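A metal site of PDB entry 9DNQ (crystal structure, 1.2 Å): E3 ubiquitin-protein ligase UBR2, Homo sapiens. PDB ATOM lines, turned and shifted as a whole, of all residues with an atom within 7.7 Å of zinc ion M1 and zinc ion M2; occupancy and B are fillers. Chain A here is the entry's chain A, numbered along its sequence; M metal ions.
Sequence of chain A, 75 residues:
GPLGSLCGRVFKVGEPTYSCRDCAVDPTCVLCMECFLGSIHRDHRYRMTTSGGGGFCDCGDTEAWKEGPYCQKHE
Zinc ion M1 is bound by ND1 of His 74, SG of Cys 59, SG of Cys 71 and SG of Cys 35. Zinc ion M1 has four donor atoms within binding distance.
SG of Cys 57 is bound to zinc ion M2, at 2.3 Å. Zinc ion M2 is bound by the side-chain sulfur (SG) of Cys 7 (2.3 Å). Zinc ion M2 is bound by the side-chain sulfur (SG) of Cys 32 (2.3 Å). Zinc ion M2 is bound by SG of Cys 35 (2.4 Å). Zinc ion M2 has four donor atoms within binding distance.
The backbone NH of Cys 59 lies close to the side-chain sulfur of Cys 57 (3.4 Å). N of Lys 73 lies close to SG of Cys 71 (3.4 Å). The backbone NH (N) of Cys 57 sits at hydrogen-bond distance from the backbone carbonyl oxygen (O) of Arg 9 (3.1 Å). SG of Cys 7 lies close to N of Arg 9 (3.7 Å).
The nearest printed residue that does not touch zinc ion M2 is Cys 59 (4.2 Å).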
ATOM      1  N   LEU A   6      18.114 -23.396  29.099  1.00  0.00           N
ATOM      2  CA  LEU A   6      19.448 -22.939  29.442  1.00  0.00           C
ATOM      3  C   LEU A   6      20.357 -22.902  28.214  1.00  0.00           C
ATOM      4  O   LEU A   6      21.141 -21.959  28.059  1.00  0.00           O
ATOM      5  CB  LEU A   6      20.031 -23.830  30.528  1.00  0.00           C
ATOM      6  CG  LEU A   6      21.424 -23.510  31.037  1.00  0.00           C
ATOM      7  CD1 LEU A   6      21.515 -22.074  31.523  1.00  0.00           C
ATOM      8  CD2 LEU A   6      21.765 -24.479  32.164  1.00  0.00           C
ATOM      9  N   CYS A   7      20.272 -23.898  27.341  1.00  0.00           N
ATOM     10  CA  CYS A   7      21.202 -23.945  26.210  1.00  0.00           C
ATOM     11  C   CYS A   7      20.799 -22.981  25.100  1.00  0.00           C
ATOM     12  O   CYS A   7      21.572 -22.098  24.705  1.00  0.00           O
ATOM     13  CB  CYS A   7      21.397 -25.374  25.712  1.00  0.00           C
ATOM     14  SG  CYS A   7      22.303 -25.451  24.155  1.00  0.00           S
ATOM     15  N   GLY A   8      19.583 -23.112  24.589  1.00  0.00           N
ATOM     16  CA  GLY A   8      19.049 -22.235  23.565  1.00  0.00           C
ATOM     17  C   GLY A   8      19.092 -22.787  22.158  1.00  0.00           C
ATOM     18  O   GLY A   8      18.424 -22.248  21.279  1.00  0.00           O
ATOM     19  N   ARG A   9      19.830 -23.877  21.937  1.00  0.00           N
ATOM     20  CA  ARG A   9      19.998 -24.413  20.596  1.00  0.00           C
ATOM     21  C   ARG A   9      18.700 -25.026  20.071  1.00  0.00           C
ATOM     22  O   ARG A   9      18.036 -25.802  20.775  1.00  0.00           O
ATOM     23  CB  ARG A   9      21.104 -25.459  20.559  1.00  0.00           C
ATOM     24  CG  ARG A   9      22.514 -24.904  20.697  1.00  0.00           C
ATOM     25  CD  ARG A   9      22.916 -23.949  19.538  1.00  0.00           C
ATOM     26  NE  ARG A   9      22.266 -24.276  18.265  1.00  0.00           N
ATOM     27  CZ  ARG A   9      22.553 -25.337  17.531  1.00  0.00           C
ATOM     28  NH1 ARG A   9      23.518 -26.180  17.864  1.00  0.00           N
ATOM     29  NH2 ARG A   9      21.832 -25.575  16.426  1.00  0.00           N
ATOM     30  N   VAL A  10      18.380 -24.696  18.831  1.00  0.00           N
ATOM     31  CA  VAL A  10      17.328 -25.323  18.050  1.00  0.00           C
ATOM     32  C   VAL A  10      18.034 -26.047  16.909  1.00  0.00           C
ATOM     33  O   VAL A  10      18.892 -25.467  16.236  1.00  0.00           O
ATOM     34  CB  VAL A  10      16.356 -24.271  17.487  1.00  0.00           C
ATOM     35  CG1 VAL A  10      15.370 -24.903  16.519  1.00  0.00           C
ATOM     36  CG2 VAL A  10      15.626 -23.574  18.620  1.00  0.00           C
ATOM     37  N   PHE A  11      17.692 -27.304  16.680  1.00  0.00           N
ATOM     38  CA  PHE A  11      18.501 -28.108  15.778  1.00  0.00           C
ATOM     39  C   PHE A  11      18.294 -27.754  14.305  1.00  0.00           C
ATOM     40  O   PHE A  11      17.170 -27.560  13.830  1.00  0.00           O
ATOM     41  CB  PHE A  11      18.270 -29.605  15.994  1.00  0.00           C
ATOM     42  CG  PHE A  11      18.637 -30.054  17.377  1.00  0.00           C
ATOM     43  CD1 PHE A  11      19.960 -30.051  17.788  1.00  0.00           C
ATOM     44  CD2 PHE A  11      17.665 -30.418  18.295  1.00  0.00           C
ATOM     45  CE1 PHE A  11      20.298 -30.432  19.074  1.00  0.00           C
ATOM     46  CE2 PHE A  11      18.003 -30.793  19.573  1.00  0.00           C
ATOM     47  CZ  PHE A  11      19.309 -30.802  19.962  1.00  0.00           C
ATOM     48  N   VAL A  30      17.152 -34.768  24.681  1.00  0.00           N
ATOM     49  CA  VAL A  30      18.334 -34.740  23.830  1.00  0.00           C
ATOM     50  C   VAL A  30      19.239 -33.581  24.215  1.00  0.00           C
ATOM     51  O   VAL A  30      18.809 -32.572  24.798  1.00  0.00           O
ATOM     52  CB  VAL A  30      17.996 -34.625  22.321  1.00  0.00           C
ATOM     53  CG1 VAL A  30      17.305 -35.883  21.823  1.00  0.00           C
ATOM     54  CG2 VAL A  30      17.193 -33.348  22.018  1.00  0.00           C
ATOM     55  N   LEU A  31      20.515 -33.733  23.876  1.00  0.00           N
ATOM     56  CA  LEU A  31      21.514 -32.686  23.989  1.00  0.00           C
ATOM     57  C   LEU A  31      22.104 -32.399  22.619  1.00  0.00           C
ATOM     58  O   LEU A  31      22.254 -33.308  21.782  1.00  0.00           O
ATOM     59  CB  LEU A  31      22.669 -33.167  24.891  1.00  0.00           C
ATOM     60  CG  LEU A  31      22.265 -33.483  26.334  1.00  0.00           C
ATOM     61  CD1 LEU A  31      23.470 -34.049  27.087  1.00  0.00           C
ATOM     62  CD2 LEU A  31      21.760 -32.258  27.051  1.00  0.00           C
ATOM     63  N   CYS A  32      22.447 -31.140  22.393  1.00  0.00           N
ATOM     64  CA  CYS A  32      23.277 -30.805  21.238  1.00  0.00           C
ATOM     65  C   CYS A  32      24.686 -31.375  21.439  1.00  0.00           C
ATOM     66  O   CYS A  32      25.070 -31.809  22.525  1.00  0.00           O
ATOM     67  CB  CYS A  32      23.359 -29.288  21.031  1.00  0.00           C
ATOM     68  SG  CYS A  32      24.297 -28.343  22.322  1.00  0.00           S
ATOM     69  N   MET A  33      25.438 -31.414  20.337  1.00  0.00           N
ATOM     70  CA  MET A  33      26.722 -32.115  20.370  1.00  0.00           C
ATOM     71  C   MET A  33      27.684 -31.485  21.393  1.00  0.00           C
ATOM     72  O   MET A  33      28.356 -32.197  22.144  1.00  0.00           O
ATOM     73  CB  MET A  33      27.325 -32.174  18.972  1.00  0.00           C
ATOM     74  CG  MET A  33      28.653 -32.912  18.940  1.00  0.00           C
ATOM     75  SD  MET A  33      29.618 -32.757  17.434  1.00  0.00           S
ATOM     76  CE  MET A  33      30.467 -31.247  17.842  1.00  0.00           C
ATOM     77  N   GLU A  34      27.748 -30.159  21.433  1.00  0.00           N
ATOM     78  CA  GLU A  34      28.672 -29.508  22.345  1.00  0.00           C
ATOM     79  C   GLU A  34      28.302 -29.788  23.790  1.00  0.00           C
ATOM     80  O   GLU A  34      29.175 -30.078  24.625  1.00  0.00           O
ATOM     81  CB  GLU A  34      28.696 -28.017  22.028  1.00  0.00           C
ATOM     82  CG  GLU A  34      29.442 -27.715  20.718  1.00  0.00           C
ATOM     83  CD  GLU A  34      28.642 -27.952  19.408  1.00  0.00           C
ATOM     84  OE1 GLU A  34      27.412 -28.282  19.395  1.00  0.00           O
ATOM     85  OE2 GLU A  34      29.270 -27.799  18.330  1.00  0.00           O
ATOM     86  N   CYS A  35      27.000 -29.751  24.111  1.00  0.00           N
ATOM     87  CA  CYS A  35      26.561 -30.110  25.454  1.00  0.00           C
ATOM     88  C   CYS A  35      26.870 -31.575  25.769  1.00  0.00           C
ATOM     89  O   CYS A  35      27.414 -31.883  26.827  1.00  0.00           O
ATOM     90  CB  CYS A  35      25.075 -29.779  25.627  1.00  0.00           C
ATOM     91  SG  CYS A  35      24.744 -28.012  25.716  1.00  0.00           S
ATOM     92  N   PHE A  36      26.576 -32.481  24.826  1.00  0.00           N
ATOM     93  CA  PHE A  36      26.783 -33.915  25.046  1.00  0.00           C
ATOM     94  C   PHE A  36      28.251 -34.209  25.310  1.00  0.00           C
ATOM     95  O   PHE A  36      28.614 -34.931  26.251  1.00  0.00           O
ATOM     96  CB  PHE A  36      26.297 -34.690  23.812  1.00  0.00           C
ATOM     97  CG  PHE A  36      26.605 -36.157  23.857  1.00  0.00           C
ATOM     98  CD1 PHE A  36      25.924 -37.000  24.719  1.00  0.00           C
ATOM     99  CD2 PHE A  36      27.615 -36.688  23.065  1.00  0.00           C
ATOM    100  CE1 PHE A  36      26.239 -38.356  24.766  1.00  0.00           C
ATOM    101  CE2 PHE A  36      27.908 -38.035  23.111  1.00  0.00           C
ATOM    102  CZ  PHE A  36      27.224 -38.865  23.958  1.00  0.00           C
ATOM    103  N   GLY A  38      30.630 -32.411  26.411  1.00  0.00           N
ATOM    104  CA  GLY A  38      31.072 -31.875  27.680  1.00  0.00           C
ATOM    105  C   GLY A  38      30.236 -32.340  28.868  1.00  0.00           C
ATOM    106  O   GLY A  38      30.231 -31.706  29.927  1.00  0.00           O
ATOM    107  N   SER A  39      29.566 -33.479  28.714  1.00  0.00           N
ATOM    108  CA  SER A  39      28.681 -34.000  29.752  1.00  0.00           C
ATOM    109  C   SER A  39      29.147 -35.381  30.204  1.00  0.00           C
ATOM    110  O   SER A  39      29.912 -36.051  29.520  1.00  0.00           O
ATOM    111  CB  SER A  39      27.241 -34.091  29.236  1.00  0.00           C
ATOM    112  OG  SER A  39      27.036 -35.298  28.512  1.00  0.00           O
ATOM    113  N   PHE A  56      14.934 -29.044  20.183  1.00  0.00           N
ATOM    114  CA  PHE A  56      15.811 -28.166  20.940  1.00  0.00           C
ATOM    115  C   PHE A  56      16.555 -28.944  22.027  1.00  0.00           C
ATOM    116  O   PHE A  56      16.123 -30.006  22.478  1.00  0.00           O
ATOM    117  CB  PHE A  56      15.054 -26.983  21.567  1.00  0.00           C
ATOM    118  CG  PHE A  56      13.944 -27.376  22.503  1.00  0.00           C
ATOM    119  CD1 PHE A  56      12.716 -27.804  22.026  1.00  0.00           C
ATOM    120  CD2 PHE A  56      14.122 -27.272  23.876  1.00  0.00           C
ATOM    121  CE1 PHE A  56      11.694 -28.154  22.896  1.00  0.00           C
ATOM    122  CE2 PHE A  56      13.087 -27.616  24.753  1.00  0.00           C
ATOM    123  CZ  PHE A  56      11.875 -28.057  24.249  1.00  0.00           C
ATOM    124  N   CYS A  57      17.701 -28.393  22.421  1.00  0.00           N
ATOM    125  CA  CYS A  57      18.571 -29.007  23.412  1.00  0.00           C
ATOM    126  C   CYS A  57      17.974 -28.888  24.822  1.00  0.00           C
ATOM    127  O   CYS A  57      17.514 -27.817  25.222  1.00  0.00           O
ATOM    128  CB  CYS A  57      19.950 -28.346  23.366  1.00  0.00           C
ATOM    129  SG  CYS A  57      21.109 -29.002  24.595  1.00  0.00           S
ATOM    130  N   ASP A  58      18.015 -30.001  25.561  1.00  0.00           N
ATOM    131  CA  ASP A  58      17.467 -30.092  26.913  1.00  0.00           C
ATOM    132  C   ASP A  58      18.548 -29.991  27.989  1.00  0.00           C
ATOM    133  O   ASP A  58      18.313 -30.428  29.132  1.00  0.00           O
ATOM    134  CB  ASP A  58      16.712 -31.412  27.065  1.00  0.00           C
ATOM    135  CG  ASP A  58      15.533 -31.532  26.131  1.00  0.00           C
ATOM    136  OD1 ASP A  58      14.652 -30.634  26.186  1.00  0.00           O
ATOM    137  OD2 ASP A  58      15.486 -32.500  25.345  1.00  0.00           O
ATOM    138  N   CYS A  59      19.712 -29.435  27.675  1.00  0.00           N
ATOM    139  CA  CYS A  59      20.728 -29.256  28.707  1.00  0.00           C
ATOM    140  C   CYS A  59      20.172 -28.414  29.841  1.00  0.00           C
ATOM    141  O   CYS A  59      19.483 -27.407  29.608  1.00  0.00           O
ATOM    142  CB  CYS A  59      21.991 -28.600  28.148  1.00  0.00           C
ATOM    143  SG  CYS A  59      23.365 -28.644  29.289  1.00  0.00           S
ATOM    144  N   GLY A  60      20.448 -28.826  31.080  1.00  0.00           N
ATOM    145  CA  GLY A  60      19.993 -28.078  32.226  1.00  0.00           C
ATOM    146  C   GLY A  60      18.562 -28.324  32.619  1.00  0.00           C
ATOM    147  O   GLY A  60      18.101 -27.732  33.601  1.00  0.00           O
ATOM    148  N   PRO A  69      22.467 -33.242  34.910  1.00  0.00           N
ATOM    149  CA  PRO A  69      21.646 -32.334  34.081  1.00  0.00           C
ATOM    150  C   PRO A  69      22.416 -31.232  33.371  1.00  0.00           C
ATOM    151  O   PRO A  69      21.894 -30.712  32.377  1.00  0.00           O
ATOM    152  CB  PRO A  69      20.649 -31.736  35.091  1.00  0.00           C
ATOM    153  CG  PRO A  69      21.382 -31.810  36.388  1.00  0.00           C
ATOM    154  CD  PRO A  69      22.123 -33.113  36.340  1.00  0.00           C
ATOM    155  N   TYR A  70      23.590 -30.837  33.839  1.00  0.00           N
ATOM    156  CA  TYR A  70      24.329 -29.696  33.288  1.00  0.00           C
ATOM    157  C   TYR A  70      25.650 -30.165  32.690  1.00  0.00           C
ATOM    158  O   TYR A  70      26.432 -30.838  33.356  1.00  0.00           O
ATOM    159  CB  TYR A  70      24.648 -28.661  34.370  1.00  0.00           C
ATOM    160  CG  TYR A  70      23.450 -28.142  35.118  1.00  0.00           C
ATOM    161  CD1 TYR A  70      22.522 -27.330  34.498  1.00  0.00           C
ATOM    162  CD2 TYR A  70      23.245 -28.489  36.444  1.00  0.00           C
ATOM    163  CE1 TYR A  70      21.403 -26.878  35.191  1.00  0.00           C
ATOM    164  CE2 TYR A  70      22.134 -28.028  37.145  1.00  0.00           C
ATOM    165  CZ  TYR A  70      21.211 -27.237  36.519  1.00  0.00           C
ATOM    166  OH  TYR A  70      20.125 -26.805  37.245  1.00  0.00           O
ATOM    167  N   CYS A  71      25.900 -29.768  31.443  1.00  0.00           N
ATOM    168  CA  CYS A  71      27.217 -29.985  30.855  1.00  0.00           C
ATOM    169  C   CYS A  71      28.197 -28.945  31.407  1.00  0.00           C
ATOM    170  O   CYS A  71      27.827 -28.024  32.133  1.00  0.00           O
ATOM    171  CB  CYS A  71      27.169 -29.875  29.334  1.00  0.00           C
ATOM    172  SG  CYS A  71      27.107 -28.174  28.717  1.00  0.00           S
ATOM    173  N   GLN A  72      29.473 -29.085  31.039  1.00  0.00           N
ATOM    174  CA  GLN A  72      30.463 -28.200  31.627  1.00  0.00           C
ATOM    175  C   GLN A  72      30.291 -26.751  31.161  1.00  0.00           C
ATOM    176  O   GLN A  72      30.499 -25.822  31.947  1.00  0.00           O
ATOM    177  CB  GLN A  72      31.876 -28.751  31.402  1.00  0.00           C
ATOM    178  CG  GLN A  72      32.964 -28.070  32.241  1.00  0.00           C
ATOM    179  CD  GLN A  72      33.720 -29.082  33.132  1.00  0.00           C
ATOM    180  OE1 GLN A  72      34.336 -30.032  32.633  1.00  0.00           O
ATOM    181  NE2 GLN A  72      33.675 -28.876  34.448  1.00  0.00           N
ATOM    182  N   LYS A  73      29.861 -26.538  29.925  1.00  0.00           N
ATOM    183  CA  LYS A  73      29.633 -25.172  29.486  1.00  0.00           C
ATOM    184  C   LYS A  73      28.486 -24.518  30.268  1.00  0.00           C
ATOM    185  O   LYS A  73      28.518 -23.309  30.531  1.00  0.00           O
ATOM    186  CB  LYS A  73      29.363 -25.180  27.981  1.00  0.00           C
ATOM    187  CG  LYS A  73      28.860 -23.872  27.402  1.00  0.00           C
ATOM    188  CD  LYS A  73      28.593 -24.052  25.918  1.00  0.00           C
ATOM    189  CE  LYS A  73      28.539 -22.732  25.190  1.00  0.00           C
ATOM    190  NZ  LYS A  73      27.179 -22.137  25.233  1.00  0.00           N
ATOM    191  N   HIS A  74      27.490 -25.310  30.648  1.00  0.00           N
ATOM    192  CA  HIS A  74      26.311 -24.819  31.356  1.00  0.00           C
ATOM    193  C   HIS A  74      26.355 -25.140  32.850  1.00  0.00           C
ATOM    194  O   HIS A  74      25.315 -25.144  33.506  1.00  0.00           O
ATOM    195  CB  HIS A  74      25.055 -25.331  30.660  1.00  0.00           C
ATOM    196  CG  HIS A  74      24.891 -24.774  29.281  1.00  0.00           C
ATOM    197  ND1 HIS A  74      24.901 -25.556  28.144  1.00  0.00           N
ATOM    198  CD2 HIS A  74      24.771 -23.493  28.862  1.00  0.00           C
ATOM    199  CE1 HIS A  74      24.779 -24.769  27.085  1.00  0.00           C
ATOM    200  NE2 HIS A  74      24.689 -23.519  27.493  1.00  0.00           N
ATOM    201  N   GLU A  75      27.553 -25.365  33.396  1.00  0.00           N
ATOM    202  CA  GLU A  75      27.669 -25.756  34.807  1.00  0.00           C
ATOM    203  C   GLU A  75      27.211 -24.638  35.745  1.00  0.00           C
ATOM    204  O   GLU A  75      26.919 -24.948  36.899  1.00  0.00           O
ATOM    205  CB  GLU A  75      29.080 -26.200  35.173  1.00  0.00           C
ATOM    206  CG  GLU A  75      30.068 -25.074  35.211  1.00  0.00           C
ATOM    207  CD  GLU A  75      31.482 -25.546  35.458  1.00  0.00           C
ATOM    208  OE1 GLU A  75      31.723 -26.770  35.444  1.00  0.00           O
ATOM    209  OE2 GLU A  75      32.360 -24.672  35.646  1.00  0.00           O
ATOM    210  OXT GLU A  75      27.139 -23.452  35.383  1.00  0.00           O
HETATM  211 ZN    ZN M   1      24.967 -27.618  28.039  1.00  0.00          ZN
HETATM  212 ZN    ZN M   2      22.963 -27.682  24.125  1.00  0.00          ZN
